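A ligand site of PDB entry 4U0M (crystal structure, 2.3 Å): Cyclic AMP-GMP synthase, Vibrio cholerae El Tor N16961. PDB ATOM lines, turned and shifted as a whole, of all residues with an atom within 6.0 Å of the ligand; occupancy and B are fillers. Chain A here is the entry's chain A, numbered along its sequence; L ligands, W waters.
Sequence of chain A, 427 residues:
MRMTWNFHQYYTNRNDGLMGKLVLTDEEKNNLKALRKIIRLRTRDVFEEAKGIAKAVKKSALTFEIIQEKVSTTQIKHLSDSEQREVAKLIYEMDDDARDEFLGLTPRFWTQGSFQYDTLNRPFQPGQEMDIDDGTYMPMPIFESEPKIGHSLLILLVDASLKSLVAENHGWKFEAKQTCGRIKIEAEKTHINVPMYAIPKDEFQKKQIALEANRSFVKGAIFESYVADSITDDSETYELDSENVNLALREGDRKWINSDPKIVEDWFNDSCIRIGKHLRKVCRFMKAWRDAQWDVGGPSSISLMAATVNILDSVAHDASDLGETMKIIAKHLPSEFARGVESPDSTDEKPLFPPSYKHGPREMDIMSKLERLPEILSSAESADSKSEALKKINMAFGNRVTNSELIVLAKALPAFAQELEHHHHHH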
ATOM      1  N   LYS A  33     -13.462  22.707  -4.685  1.00  0.00           N
ATOM      2  CA  LYS A  33     -14.851  22.731  -5.138  1.00  0.00           C
ATOM      3  C   LYS A  33     -14.963  23.444  -6.476  1.00  0.00           C
ATOM      4  O   LYS A  33     -15.715  23.022  -7.360  1.00  0.00           O
ATOM      5  CB  LYS A  33     -15.756  23.395  -4.103  1.00  0.00           C
ATOM      6  CG  LYS A  33     -15.940  22.592  -2.835  1.00  0.00           C
ATOM      7  CD  LYS A  33     -16.979  23.231  -1.921  1.00  0.00           C
ATOM      8  CE  LYS A  33     -17.259  22.371  -0.702  1.00  0.00           C
ATOM      9  NZ  LYS A  33     -18.309  22.959   0.164  1.00  0.00           N
ATOM     10  N   ARG A  36     -13.542  21.194  -9.197  1.00  0.00           N
ATOM     11  CA  ARG A  36     -14.492  20.136  -9.520  1.00  0.00           C
ATOM     12  C   ARG A  36     -15.635  20.675 -10.379  1.00  0.00           C
ATOM     13  O   ARG A  36     -16.113  20.006 -11.296  1.00  0.00           O
ATOM     14  CB  ARG A  36     -15.045  19.506  -8.246  1.00  0.00           C
ATOM     15  CG  ARG A  36     -16.111  18.454  -8.481  1.00  0.00           C
ATOM     16  CD  ARG A  36     -16.619  17.878  -7.168  1.00  0.00           C
ATOM     17  NE  ARG A  36     -17.158  18.904  -6.284  1.00  0.00           N
ATOM     18  CZ  ARG A  36     -17.703  18.668  -5.102  1.00  0.00           C
ATOM     19  NH1 ARG A  36     -17.777  17.431  -4.633  1.00  0.00           N
ATOM     20  NH2 ARG A  36     -18.165  19.672  -4.361  1.00  0.00           N
ATOM     21  N   ARG A  40     -16.755  19.434 -14.192  1.00  0.00           N
ATOM     22  CA  ARG A  40     -18.114  18.956 -14.413  1.00  0.00           C
ATOM     23  C   ARG A  40     -18.789  19.711 -15.555  1.00  0.00           C
ATOM     24  O   ARG A  40     -19.453  19.108 -16.409  1.00  0.00           O
ATOM     25  CB  ARG A  40     -18.954  19.070 -13.138  1.00  0.00           C
ATOM     26  CG  ARG A  40     -18.536  18.092 -12.042  1.00  0.00           C
ATOM     27  CD  ARG A  40     -19.458  18.192 -10.839  1.00  0.00           C
ATOM     28  NE  ARG A  40     -19.145  17.179  -9.838  1.00  0.00           N
ATOM     29  CZ  ARG A  40     -19.810  17.018  -8.695  1.00  0.00           C
ATOM     30  NH1 ARG A  40     -20.818  17.820  -8.402  1.00  0.00           N
ATOM     31  NH2 ARG A  40     -19.460  16.066  -7.844  1.00  0.00           N
ATOM     32  N   ARG A  44     -19.725  18.038 -19.360  1.00  0.00           N
ATOM     33  CA  ARG A  44     -21.095  18.051 -19.867  1.00  0.00           C
ATOM     34  C   ARG A  44     -21.186  18.775 -21.205  1.00  0.00           C
ATOM     35  O   ARG A  44     -21.916  18.356 -22.096  1.00  0.00           O
ATOM     36  CB  ARG A  44     -22.051  18.680 -18.847  1.00  0.00           C
ATOM     37  CG  ARG A  44     -22.392  17.783 -17.673  1.00  0.00           C
ATOM     38  CD  ARG A  44     -23.590  18.312 -16.900  1.00  0.00           C
ATOM     39  NE  ARG A  44     -23.281  19.544 -16.183  1.00  0.00           N
ATOM     40  CZ  ARG A  44     -23.093  19.618 -14.865  1.00  0.00           C
ATOM     41  NH1 ARG A  44     -23.213  18.526 -14.118  1.00  0.00           N
ATOM     42  NH2 ARG A  44     -22.815  20.785 -14.294  1.00  0.00           N
ATOM     43  N   PRO A 107     -24.315  12.583 -18.578  1.00  0.00           N
ATOM     44  CA  PRO A 107     -23.191  12.399 -17.637  1.00  0.00           C
ATOM     45  C   PRO A 107     -23.494  12.978 -16.263  1.00  0.00           C
ATOM     46  O   PRO A 107     -23.804  14.163 -16.160  1.00  0.00           O
ATOM     47  CB  PRO A 107     -22.049  13.187 -18.292  1.00  0.00           C
ATOM     48  CG  PRO A 107     -22.431  13.360 -19.703  1.00  0.00           C
ATOM     49  CD  PRO A 107     -23.926  13.400 -19.734  1.00  0.00           C
ATOM     50  N   ARG A 108     -23.393  12.156 -15.229  1.00  0.00           N
ATOM     51  CA  ARG A 108     -23.615  12.619 -13.857  1.00  0.00           C
ATOM     52  C   ARG A 108     -22.310  12.563 -13.071  1.00  0.00           C
ATOM     53  O   ARG A 108     -21.354  11.918 -13.501  1.00  0.00           O
ATOM     54  CB  ARG A 108     -24.693  11.782 -13.178  1.00  0.00           C
ATOM     55  CG  ARG A 108     -25.861  11.411 -14.076  1.00  0.00           C
ATOM     56  CD  ARG A 108     -26.624  12.628 -14.557  1.00  0.00           C
ATOM     57  NE  ARG A 108     -27.438  13.234 -13.505  1.00  0.00           N
ATOM     58  CZ  ARG A 108     -28.352  14.171 -13.716  1.00  0.00           C
ATOM     59  NH1 ARG A 108     -28.574  14.626 -14.934  1.00  0.00           N
ATOM     60  NH2 ARG A 108     -29.051  14.664 -12.690  1.00  0.00           N
ATOM     61  N   PHE A 109     -22.275  13.232 -11.931  1.00  0.00           N
ATOM     62  CA  PHE A 109     -21.058  13.281 -11.126  1.00  0.00           C
ATOM     63  C   PHE A 109     -21.327  13.023  -9.641  1.00  0.00           C
ATOM     64  O   PHE A 109     -22.387  13.384  -9.122  1.00  0.00           O
ATOM     65  CB  PHE A 109     -20.350  14.615 -11.298  1.00  0.00           C
ATOM     66  CG  PHE A 109     -20.103  14.987 -12.733  1.00  0.00           C
ATOM     67  CD1 PHE A 109     -18.967  14.546 -13.402  1.00  0.00           C
ATOM     68  CD2 PHE A 109     -21.018  15.774 -13.428  1.00  0.00           C
ATOM     69  CE1 PHE A 109     -18.745  14.883 -14.721  1.00  0.00           C
ATOM     70  CE2 PHE A 109     -20.795  16.111 -14.747  1.00  0.00           C
ATOM     71  CZ  PHE A 109     -19.665  15.666 -15.393  1.00  0.00           C
ATOM     72  N   TRP A 110     -20.366  12.399  -8.983  1.00  0.00           N
ATOM     73  CA  TRP A 110     -20.429  12.204  -7.534  1.00  0.00           C
ATOM     74  C   TRP A 110     -19.035  11.976  -6.978  1.00  0.00           C
ATOM     75  O   TRP A 110     -18.313  11.085  -7.410  1.00  0.00           O
ATOM     76  CB  TRP A 110     -21.337  11.020  -7.191  1.00  0.00           C
ATOM     77  CG  TRP A 110     -21.911  11.102  -5.814  1.00  0.00           C
ATOM     78  CD1 TRP A 110     -21.275  10.813  -4.639  1.00  0.00           C
ATOM     79  CD2 TRP A 110     -23.249  11.485  -5.466  1.00  0.00           C
ATOM     80  NE1 TRP A 110     -22.131  11.004  -3.580  1.00  0.00           N
ATOM     81  CE2 TRP A 110     -23.345  11.411  -4.059  1.00  0.00           C
ATOM     82  CE3 TRP A 110     -24.363  11.880  -6.205  1.00  0.00           C
ATOM     83  CZ2 TRP A 110     -24.527  11.722  -3.380  1.00  0.00           C
ATOM     84  CZ3 TRP A 110     -25.530  12.190  -5.526  1.00  0.00           C
ATOM     85  CH2 TRP A 110     -25.606  12.112  -4.131  1.00  0.00           C
ATOM     86  N   THR A 111     -18.656  12.798  -6.005  1.00  0.00           N
ATOM     87  CA  THR A 111     -17.326  12.727  -5.417  1.00  0.00           C
ATOM     88  C   THR A 111     -17.169  11.545  -4.461  1.00  0.00           C
ATOM     89  O   THR A 111     -18.037  11.286  -3.635  1.00  0.00           O
ATOM     90  CB  THR A 111     -16.964  14.025  -4.678  1.00  0.00           C
ATOM     91  OG1 THR A 111     -16.917  15.113  -5.613  1.00  0.00           O
ATOM     92  CG2 THR A 111     -15.603  13.893  -3.996  1.00  0.00           C
ATOM     93  N   PHE A 115     -12.364  13.405   0.287  1.00  0.00           N
ATOM     94  CA  PHE A 115     -13.091  14.658   0.204  1.00  0.00           C
ATOM     95  C   PHE A 115     -14.564  14.434   0.522  1.00  0.00           C
ATOM     96  O   PHE A 115     -15.238  15.337   1.033  1.00  0.00           O
ATOM     97  CB  PHE A 115     -12.926  15.289  -1.184  1.00  0.00           C
ATOM     98  CG  PHE A 115     -13.407  16.713  -1.251  1.00  0.00           C
ATOM     99  CD1 PHE A 115     -12.544  17.767  -0.982  1.00  0.00           C
ATOM    100  CD2 PHE A 115     -14.717  17.005  -1.584  1.00  0.00           C
ATOM    101  CE1 PHE A 115     -12.978  19.079  -1.037  1.00  0.00           C
ATOM    102  CE2 PHE A 115     -15.158  18.314  -1.650  1.00  0.00           C
ATOM    103  CZ  PHE A 115     -14.289  19.346  -1.371  1.00  0.00           C
ATOM    104  N   GLN A 116     -15.057  13.242   0.220  1.00  0.00           N
ATOM    105  CA  GLN A 116     -16.451  12.902   0.485  1.00  0.00           C
ATOM    106  C   GLN A 116     -16.694  12.578   1.955  1.00  0.00           C
ATOM    107  O   GLN A 116     -17.632  13.103   2.560  1.00  0.00           O
ATOM    108  CB  GLN A 116     -16.901  11.733  -0.402  1.00  0.00           C
ATOM    109  CG  GLN A 116     -18.379  11.380  -0.261  1.00  0.00           C
ATOM    110  CD  GLN A 116     -19.286  12.553  -0.622  1.00  0.00           C
ATOM    111  OE1 GLN A 116     -19.830  13.217   0.263  1.00  0.00           O
ATOM    112  NE2 GLN A 116     -19.447  12.796  -1.913  1.00  0.00           N
ATOM    113  N   ASP A 134     -13.526  12.710  -8.081  1.00  0.00           N
ATOM    114  CA  ASP A 134     -14.847  13.008  -8.639  1.00  0.00           C
ATOM    115  C   ASP A 134     -15.182  12.077  -9.802  1.00  0.00           C
ATOM    116  O   ASP A 134     -14.692  12.264 -10.913  1.00  0.00           O
ATOM    117  CB  ASP A 134     -14.920  14.463  -9.100  1.00  0.00           C
ATOM    118  CG  ASP A 134     -16.336  14.912  -9.383  1.00  0.00           C
ATOM    119  OD1 ASP A 134     -17.254  14.509  -8.628  1.00  0.00           O
ATOM    120  OD2 ASP A 134     -16.550  15.671 -10.355  1.00  0.00           O
ATOM    121  N   TYR A 137     -20.553   9.361 -13.942  1.00  0.00           N
ATOM    122  CA  TYR A 137     -21.470   8.250 -14.128  1.00  0.00           C
ATOM    123  C   TYR A 137     -22.219   8.334 -15.454  1.00  0.00           C
ATOM    124  O   TYR A 137     -22.755   9.385 -15.819  1.00  0.00           O
ATOM    125  CB  TYR A 137     -22.464   8.185 -12.966  1.00  0.00           C
ATOM    126  CG  TYR A 137     -21.808   7.834 -11.644  1.00  0.00           C
ATOM    127  CD1 TYR A 137     -21.138   8.799 -10.906  1.00  0.00           C
ATOM    128  CD2 TYR A 137     -21.861   6.542 -11.137  1.00  0.00           C
ATOM    129  CE1 TYR A 137     -20.544   8.503  -9.700  1.00  0.00           C
ATOM    130  CE2 TYR A 137     -21.267   6.229  -9.926  1.00  0.00           C
ATOM    131  CZ  TYR A 137     -20.605   7.208  -9.222  1.00  0.00           C
ATOM    132  OH  TYR A 137     -20.004   6.899  -8.017  1.00  0.00           O
ATOM    133  N   ILE A 199     -23.808   2.842 -15.135  1.00  0.00           N
ATOM    134  CA  ILE A 199     -24.905   2.450 -14.262  1.00  0.00           C
ATOM    135  C   ILE A 199     -26.196   2.264 -15.044  1.00  0.00           C
ATOM    136  O   ILE A 199     -26.351   2.827 -16.130  1.00  0.00           O
ATOM    137  CB  ILE A 199     -25.142   3.497 -13.149  1.00  0.00           C
ATOM    138  CG1 ILE A 199     -25.502   4.847 -13.761  1.00  0.00           C
ATOM    139  CG2 ILE A 199     -23.905   3.617 -12.273  1.00  0.00           C
ATOM    140  CD1 ILE A 199     -25.735   5.932 -12.734  1.00  0.00           C
ATOM    141  N   PHE A 204     -31.707   4.255 -12.632  1.00  0.00           N
ATOM    142  CA  PHE A 204     -31.238   5.612 -12.364  1.00  0.00           C
ATOM    143  C   PHE A 204     -32.372   6.619 -12.464  1.00  0.00           C
ATOM    144  O   PHE A 204     -32.528   7.482 -11.598  1.00  0.00           O
ATOM    145  CB  PHE A 204     -30.112   5.986 -13.332  1.00  0.00           C
ATOM    146  CG  PHE A 204     -29.915   7.471 -13.493  1.00  0.00           C
ATOM    147  CD1 PHE A 204     -29.207   8.188 -12.545  1.00  0.00           C
ATOM    148  CD2 PHE A 204     -30.429   8.134 -14.593  1.00  0.00           C
ATOM    149  CE1 PHE A 204     -29.028   9.551 -12.691  1.00  0.00           C
ATOM    150  CE2 PHE A 204     -30.249   9.497 -14.739  1.00  0.00           C
ATOM    151  CZ  PHE A 204     -29.549  10.209 -13.785  1.00  0.00           C
ATOM    152  N   GLN A 208     -34.158   8.704  -9.406  1.00  0.00           N
ATOM    153  CA  GLN A 208     -34.083  10.149  -9.568  1.00  0.00           C
ATOM    154  C   GLN A 208     -35.466  10.786  -9.453  1.00  0.00           C
ATOM    155  O   GLN A 208     -35.622  11.841  -8.858  1.00  0.00           O
ATOM    156  CB  GLN A 208     -33.442  10.509 -10.906  1.00  0.00           C
ATOM    157  CG  GLN A 208     -33.046  11.978 -11.031  1.00  0.00           C
ATOM    158  CD  GLN A 208     -31.911  12.345 -10.091  1.00  0.00           C
ATOM    159  OE1 GLN A 208     -31.172  11.485  -9.615  1.00  0.00           O
ATOM    160  NE2 GLN A 208     -31.756  13.640  -9.827  1.00  0.00           N
ATOM    161  N   TYR A 238     -29.880   7.801  -3.301  1.00  0.00           N
ATOM    162  CA  TYR A 238     -30.554   6.513  -3.192  1.00  0.00           C
ATOM    163  C   TYR A 238     -29.807   5.482  -4.023  1.00  0.00           C
ATOM    164  O   TYR A 238     -29.968   5.416  -5.237  1.00  0.00           O
ATOM    165  CB  TYR A 238     -32.012   6.630  -3.662  1.00  0.00           C
ATOM    166  CG  TYR A 238     -32.934   5.555  -3.113  1.00  0.00           C
ATOM    167  CD1 TYR A 238     -32.493   4.638  -2.168  1.00  0.00           C
ATOM    168  CD2 TYR A 238     -34.248   5.457  -3.562  1.00  0.00           C
ATOM    169  CE1 TYR A 238     -33.337   3.663  -1.677  1.00  0.00           C
ATOM    170  CE2 TYR A 238     -35.099   4.488  -3.077  1.00  0.00           C
ATOM    171  CZ  TYR A 238     -34.637   3.582  -2.132  1.00  0.00           C
ATOM    172  OH  TYR A 238     -35.488   2.613  -1.646  1.00  0.00           O
ATOM    173  N   GLU A 239     -28.979   4.690  -3.346  1.00  0.00           N
ATOM    174  CA  GLU A 239     -28.086   3.734  -4.008  1.00  0.00           C
ATOM    175  C   GLU A 239     -28.795   2.793  -4.974  1.00  0.00           C
ATOM    176  O   GLU A 239     -29.909   2.338  -4.715  1.00  0.00           O
ATOM    177  CB  GLU A 239     -27.324   2.934  -2.947  1.00  0.00           C
ATOM    178  CG  GLU A 239     -26.959   1.523  -3.372  1.00  0.00           C
ATOM    179  CD  GLU A 239     -26.855   0.574  -2.186  1.00  0.00           C
ATOM    180  OE1 GLU A 239     -27.262   0.969  -1.073  1.00  0.00           O
ATOM    181  OE2 GLU A 239     -26.377  -0.565  -2.365  1.00  0.00           O
ATOM    182  N   LEU A 240     -28.144   2.522  -6.107  1.00  0.00           N
ATOM    183  CA  LEU A 240     -28.670   1.617  -7.121  1.00  0.00           C
ATOM    184  C   LEU A 240     -28.186   0.199  -6.847  1.00  0.00           C
ATOM    185  O   LEU A 240     -27.577  -0.073  -5.809  1.00  0.00           O
ATOM    186  CB  LEU A 240     -28.199   2.050  -8.507  1.00  0.00           C
ATOM    187  CG  LEU A 240     -28.367   3.521  -8.882  1.00  0.00           C
ATOM    188  CD1 LEU A 240     -27.456   3.887 -10.036  1.00  0.00           C
ATOM    189  CD2 LEU A 240     -29.820   3.826  -9.237  1.00  0.00           C
ATOM    190  N   ASP A 241     -28.446  -0.713  -7.776  1.00  0.00           N
ATOM    191  CA  ASP A 241     -27.989  -2.089  -7.655  1.00  0.00           C
ATOM    192  C   ASP A 241     -26.474  -2.150  -7.781  1.00  0.00           C
ATOM    193  O   ASP A 241     -25.923  -1.885  -8.852  1.00  0.00           O
ATOM    194  CB  ASP A 241     -28.657  -2.980  -8.691  1.00  0.00           C
ATOM    195  CG  ASP A 241     -28.410  -4.451  -8.441  1.00  0.00           C
ATOM    196  OD1 ASP A 241     -28.132  -4.825  -7.286  1.00  0.00           O
ATOM    197  OD2 ASP A 241     -28.505  -5.250  -9.403  1.00  0.00           O
ATOM    198  N   SER A 242     -25.803  -2.519  -6.685  1.00  0.00           N
ATOM    199  CA  SER A 242     -24.347  -2.510  -6.616  1.00  0.00           C
ATOM    200  C   SER A 242     -23.677  -3.360  -7.698  1.00  0.00           C
ATOM    201  O   SER A 242     -22.599  -3.015  -8.190  1.00  0.00           O
ATOM    202  CB  SER A 242     -23.877  -2.979  -5.236  1.00  0.00           C
ATOM    203  OG  SER A 242     -22.464  -3.001  -5.154  1.00  0.00           O
ATOM    204  N   VAL A 245     -22.895  -1.496 -11.067  1.00  0.00           N
ATOM    205  CA  VAL A 245     -22.029  -0.327 -11.102  1.00  0.00           C
ATOM    206  C   VAL A 245     -20.652  -0.743 -11.626  1.00  0.00           C
ATOM    207  O   VAL A 245     -19.833  -1.288 -10.878  1.00  0.00           O
ATOM    208  CB  VAL A 245     -21.869   0.322  -9.713  1.00  0.00           C
ATOM    209  CG1 VAL A 245     -20.934   1.506  -9.791  1.00  0.00           C
ATOM    210  CG2 VAL A 245     -23.232   0.746  -9.184  1.00  0.00           C
ATOM    211  N   ASP A 260     -18.001  -0.990  -7.076  1.00  0.00           N
ATOM    212  CA  ASP A 260     -18.898   0.035  -6.557  1.00  0.00           C
ATOM    213  C   ASP A 260     -18.264   0.797  -5.396  1.00  0.00           C
ATOM    214  O   ASP A 260     -18.045   0.252  -4.324  1.00  0.00           O
ATOM    215  CB  ASP A 260     -20.229  -0.594  -6.113  1.00  0.00           C
ATOM    216  CG  ASP A 260     -21.226   0.435  -5.623  1.00  0.00           C
ATOM    217  OD1 ASP A 260     -20.962   1.637  -5.813  1.00  0.00           O
ATOM    218  OD2 ASP A 260     -22.259   0.037  -5.048  1.00  0.00           O
ATOM    219  N   PRO A 261     -17.970   2.089  -5.625  1.00  0.00           N
ATOM    220  CA  PRO A 261     -17.333   2.957  -4.623  1.00  0.00           C
ATOM    221  C   PRO A 261     -18.265   3.262  -3.458  1.00  0.00           C
ATOM    222  O   PRO A 261     -17.808   3.719  -2.408  1.00  0.00           O
ATOM    223  CB  PRO A 261     -17.039   4.233  -5.413  1.00  0.00           C
ATOM    224  CG  PRO A 261     -18.075   4.254  -6.479  1.00  0.00           C
ATOM    225  CD  PRO A 261     -18.290   2.822  -6.871  1.00  0.00           C
ATOM    226  N   LYS A 262     -19.557   3.001  -3.641  1.00  0.00           N
ATOM    227  CA  LYS A 262     -20.539   3.262  -2.598  1.00  0.00           C
ATOM    228  C   LYS A 262     -20.367   2.263  -1.451  1.00  0.00           C
ATOM    229  O   LYS A 262     -20.755   2.546  -0.307  1.00  0.00           O
ATOM    230  CB  LYS A 262     -21.957   3.180  -3.157  1.00  0.00           C
ATOM    231  CG  LYS A 262     -22.998   3.936  -2.349  1.00  0.00           C
ATOM    232  CD  LYS A 262     -22.708   5.422  -2.352  1.00  0.00           C
ATOM    233  CE  LYS A 262     -23.779   6.206  -1.612  1.00  0.00           C
ATOM    234  NZ  LYS A 262     -23.505   7.668  -1.633  1.00  0.00           N
ATOM    235  N   ILE A 263     -19.804   1.104  -1.762  1.00  0.00           N
ATOM    236  CA  ILE A 263     -19.562   0.070  -0.758  1.00  0.00           C
ATOM    237  C   ILE A 263     -18.587   0.570   0.303  1.00  0.00           C
ATOM    238  O   ILE A 263     -18.791   0.354   1.492  1.00  0.00           O
ATOM    239  CB  ILE A 263     -18.991  -1.211  -1.392  1.00  0.00           C
ATOM    240  CG1 ILE A 263     -19.940  -1.743  -2.478  1.00  0.00           C
ATOM    241  CG2 ILE A 263     -18.733  -2.264  -0.332  1.00  0.00           C
ATOM    242  CD1 ILE A 263     -21.287  -2.170  -1.935  1.00  0.00           C
ATOM    243  N   GLU A 265     -17.729   3.817   0.887  1.00  0.00           N
ATOM    244  CA  GLU A 265     -18.253   5.018   1.539  1.00  0.00           C
ATOM    245  C   GLU A 265     -19.230   4.668   2.645  1.00  0.00           C
ATOM    246  O   GLU A 265     -19.144   5.205   3.756  1.00  0.00           O
ATOM    247  CB  GLU A 265     -18.924   5.945   0.518  1.00  0.00           C
ATOM    248  CG  GLU A 265     -19.511   7.202   1.134  1.00  0.00           C
ATOM    249  CD  GLU A 265     -20.226   8.073   0.125  1.00  0.00           C
ATOM    250  OE1 GLU A 265     -20.182   7.746  -1.078  1.00  0.00           O
ATOM    251  OE2 GLU A 265     -20.838   9.087   0.532  1.00  0.00           O
HETATM  252  O1  LIG L   1     -24.317  15.304 -11.914  1.00  0.00           O
HETATM  253  C1  LIG L   1     -24.622  16.194 -11.086  1.00  0.00           C
HETATM  254  O2  LIG L   1     -24.555  17.411 -11.410  1.00  0.00           O
HETATM  255  C2  LIG L   1     -25.056  15.813  -9.706  1.00  0.00           C
HETATM  256  C3  LIG L   1     -24.034  16.309  -8.693  1.00  0.00           C
HETATM  257  C4  LIG L   1     -24.185  15.544  -7.362  1.00  0.00           C
HETATM  258  C5  LIG L   1     -23.235  16.168  -6.313  1.00  0.00           C
HETATM  259  O3  LIG L   1     -22.553  17.118  -6.623  1.00  0.00           O
HETATM  260  N1  LIG L   1     -25.133  14.387  -9.601  1.00  0.00           N
HETATM  261  C6  LIG L   1     -26.342  13.657  -9.936  1.00  0.00           C
HETATM  262  O4  LIG L   1     -27.340  14.246 -10.310  1.00  0.00           O
HETATM  263  C7  LIG L   1     -26.329  12.133  -9.792  1.00  0.00           C
HETATM  264  C8  LIG L   1     -24.999  11.404  -9.763  1.00  0.00           C
HETATM  265  C9  LIG L   1     -24.966  10.050  -9.632  1.00  0.00           C
HETATM  266  C10 LIG L   1     -26.261   9.266  -9.519  1.00  0.00           C
HETATM  267  C11 LIG L   1     -27.453   9.908  -9.546  1.00  0.00           C
HETATM  268  C12 LIG L   1     -27.494  11.434  -9.688  1.00  0.00           C
HETATM  269  N2  LIG L   1     -26.217   7.830  -9.380  1.00  0.00           N
HETATM  270  C13 LIG L   1     -25.120   7.205  -8.700  1.00  0.00           C
HETATM  271  C14 LIG L   1     -25.048   7.675  -7.249  1.00  0.00           C
HETATM  272  N3  LIG L   1     -23.954   7.010  -6.599  1.00  0.00           N
HETATM  273  C15 LIG L   1     -26.298   7.312  -6.500  1.00  0.00           C
HETATM  274  N4  LIG L   1     -26.418   5.912  -6.260  1.00  0.00           N
HETATM  275  C16 LIG L   1     -25.268   5.079  -6.225  1.00  0.00           C
HETATM  276  C17 LIG L   1     -24.069   5.590  -6.399  1.00  0.00           C
HETATM  277  N5  LIG L   1     -25.345   3.727  -6.037  1.00  0.00           N
HETATM  278  C18 LIG L   1     -24.383   2.753  -5.979  1.00  0.00           C
HETATM  279  N6  LIG L   1     -24.723   1.381  -5.774  1.00  0.00           N
HETATM  280  N7  LIG L   1     -23.117   3.147  -6.138  1.00  0.00           N
HETATM  281  C19 LIG L   1     -22.839   4.607  -6.355  1.00  0.00           C
HETATM  282  O5  LIG L   1     -21.529   5.073  -6.531  1.00  0.00           O
HETATM  283  N8  LIG L   1     -23.146  15.603  -4.987  1.00  0.00           N
HETATM  284  C20 LIG L   1     -22.252  16.178  -4.035  1.00  0.00           C
HETATM  285  C21 LIG L   1     -20.928  15.479  -4.160  1.00  0.00           C
HETATM  286  O6  LIG L   1     -20.015  15.692  -3.313  1.00  0.00           O
HETATM  287  O7  LIG L   1     -20.724  14.677  -5.097  1.00  0.00           O
HETATM  288  C22 LIG L   1     -22.811  16.034  -2.625  1.00  0.00           C
HETATM  289  C23 LIG L   1     -23.270  17.394  -2.058  1.00  0.00           C
HETATM  290  C24 LIG L   1     -22.140  18.432  -2.110  1.00  0.00           C
HETATM  291  O8  LIG L   1     -22.407  19.665  -2.175  1.00  0.00           O
HETATM  292  O9  LIG L   1     -20.926  18.067  -2.104  1.00  0.00           O
HETATM  293  C25 LIG L   1     -22.803   7.725  -6.140  1.00  0.00           C
HETATM  294  O   HOH W   1     -29.114   6.877  -8.460  1.00  0.00           O
HETATM  295  O   HOH W   2     -24.440  19.560  -6.597  1.00  0.00           O
HETATM  296  O   HOH W   3     -23.446  19.393 -10.050  1.00  0.00           O
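O of Arg 108 lies within hydrogen-bond range of N of Tyr 137 (2.7 Å).
N of Lys 262 sits at hydrogen-bond distance from OD1 of Asp 260, 2.9 Å away.
The guanidinium group of Arg 36 lies within hydrogen-bond range of the side-chain hydroxyl of Thr 111.
The guanidinium group of Arg 40 lies within salt-bridge range of the side-chain carboxylate of Asp 134, at 2.8 Å.
OD2 of Asp 260 lies within hydrogen-bond range of OG of Ser 242, at 3.0 Å.
O of Thr 111 lies within hydrogen-bond range of NE2 of Gln 116 (2.7 Å).
OG1 of Thr 111 lies within hydrogen-bond range of OD1 of Asp 134 (3.1 Å).
NZ of Lys 262 is in salt-bridge range of OE1 of Glu 265 (3.4 Å).
O of Leu 240 sits at hydrogen-bond distance from N6 of the ligand (3.2 Å).
An oxygen (O2) of the ligand lies within salt-bridge range of the guanidinium group (NH1) of Arg 44, at 3.2 Å.
N of Thr 111 lies within hydrogen-bond range of O7 of the ligand (2.9 Å).
The backbone NH of Phe 109 is in hydrogen-bond range of an oxygen (O1) of the ligand.
NH2 of Arg 40 lies within salt-bridge range of O7 of the ligand, 3.3 Å away.
OH of Tyr 137 is in hydrogen-bond range of O5 of the ligand (2.8 Å).
NH1 of Arg 36 lies within salt-bridge range of O6 of the ligand.
An oxygen (O4) of the ligand lies within hydrogen-bond range of the guanidinium group (NH2) of Arg 108 (3.0 Å).
A nitrogen (N5) of the ligand lies within hydrogen-bond range of the backbone NH of Leu 240 (3.0 Å).
An oxygen (O6) of the ligand sits at hydrogen-bond distance from the side-chain amide nitrogen (NE2) of Gln 116, 3.3 Å away.
N1 of the ligand is in hydrogen-bond range of O of Phe 109, 3.0 Å away.
A nitrogen (N7) of the ligand is in hydrogen-bond range of the side-chain carboxylate of Asp 260.
CA of Trp 110 touches O7 of the ligand (3.5 Å).
Ile 199 touches the ligand (CD1 to N2, 3.9 Å).
CE1 of Phe 204 touches C11 of the ligand, at 3.5 Å.
Gln 208 touches the ligand.
Tyr 238 touches the ligand (O to N4, 3.7 Å).
CG of Glu 239 touches N6 of the ligand (3.3 Å).
CA of Ser 242 touches N6 of the ligand, 3.999 Å away.
CG2 of Val 245 touches N6 of the ligand (3.8 Å).
Pro 261 touches the ligand (CG to O5, 3.6 Å).
CB of Lys 262 touches N7 of the ligand, at 3.2 Å.
Hydrophobic or aromatic side chains within 4 Å of the ligand: Phe 109, Trp 110, Tyr 137, Ile 199, Phe 204, Val 245 and Pro 261.
Of the 27 residues printed, 20 come within 4 Å of the ligand.
Along chain A the residues within 4 Å of the ligand span positions 36 to 262.
Water W3 lies within hydrogen-bond range of O2 of the ligand and NH1 of Arg 40.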
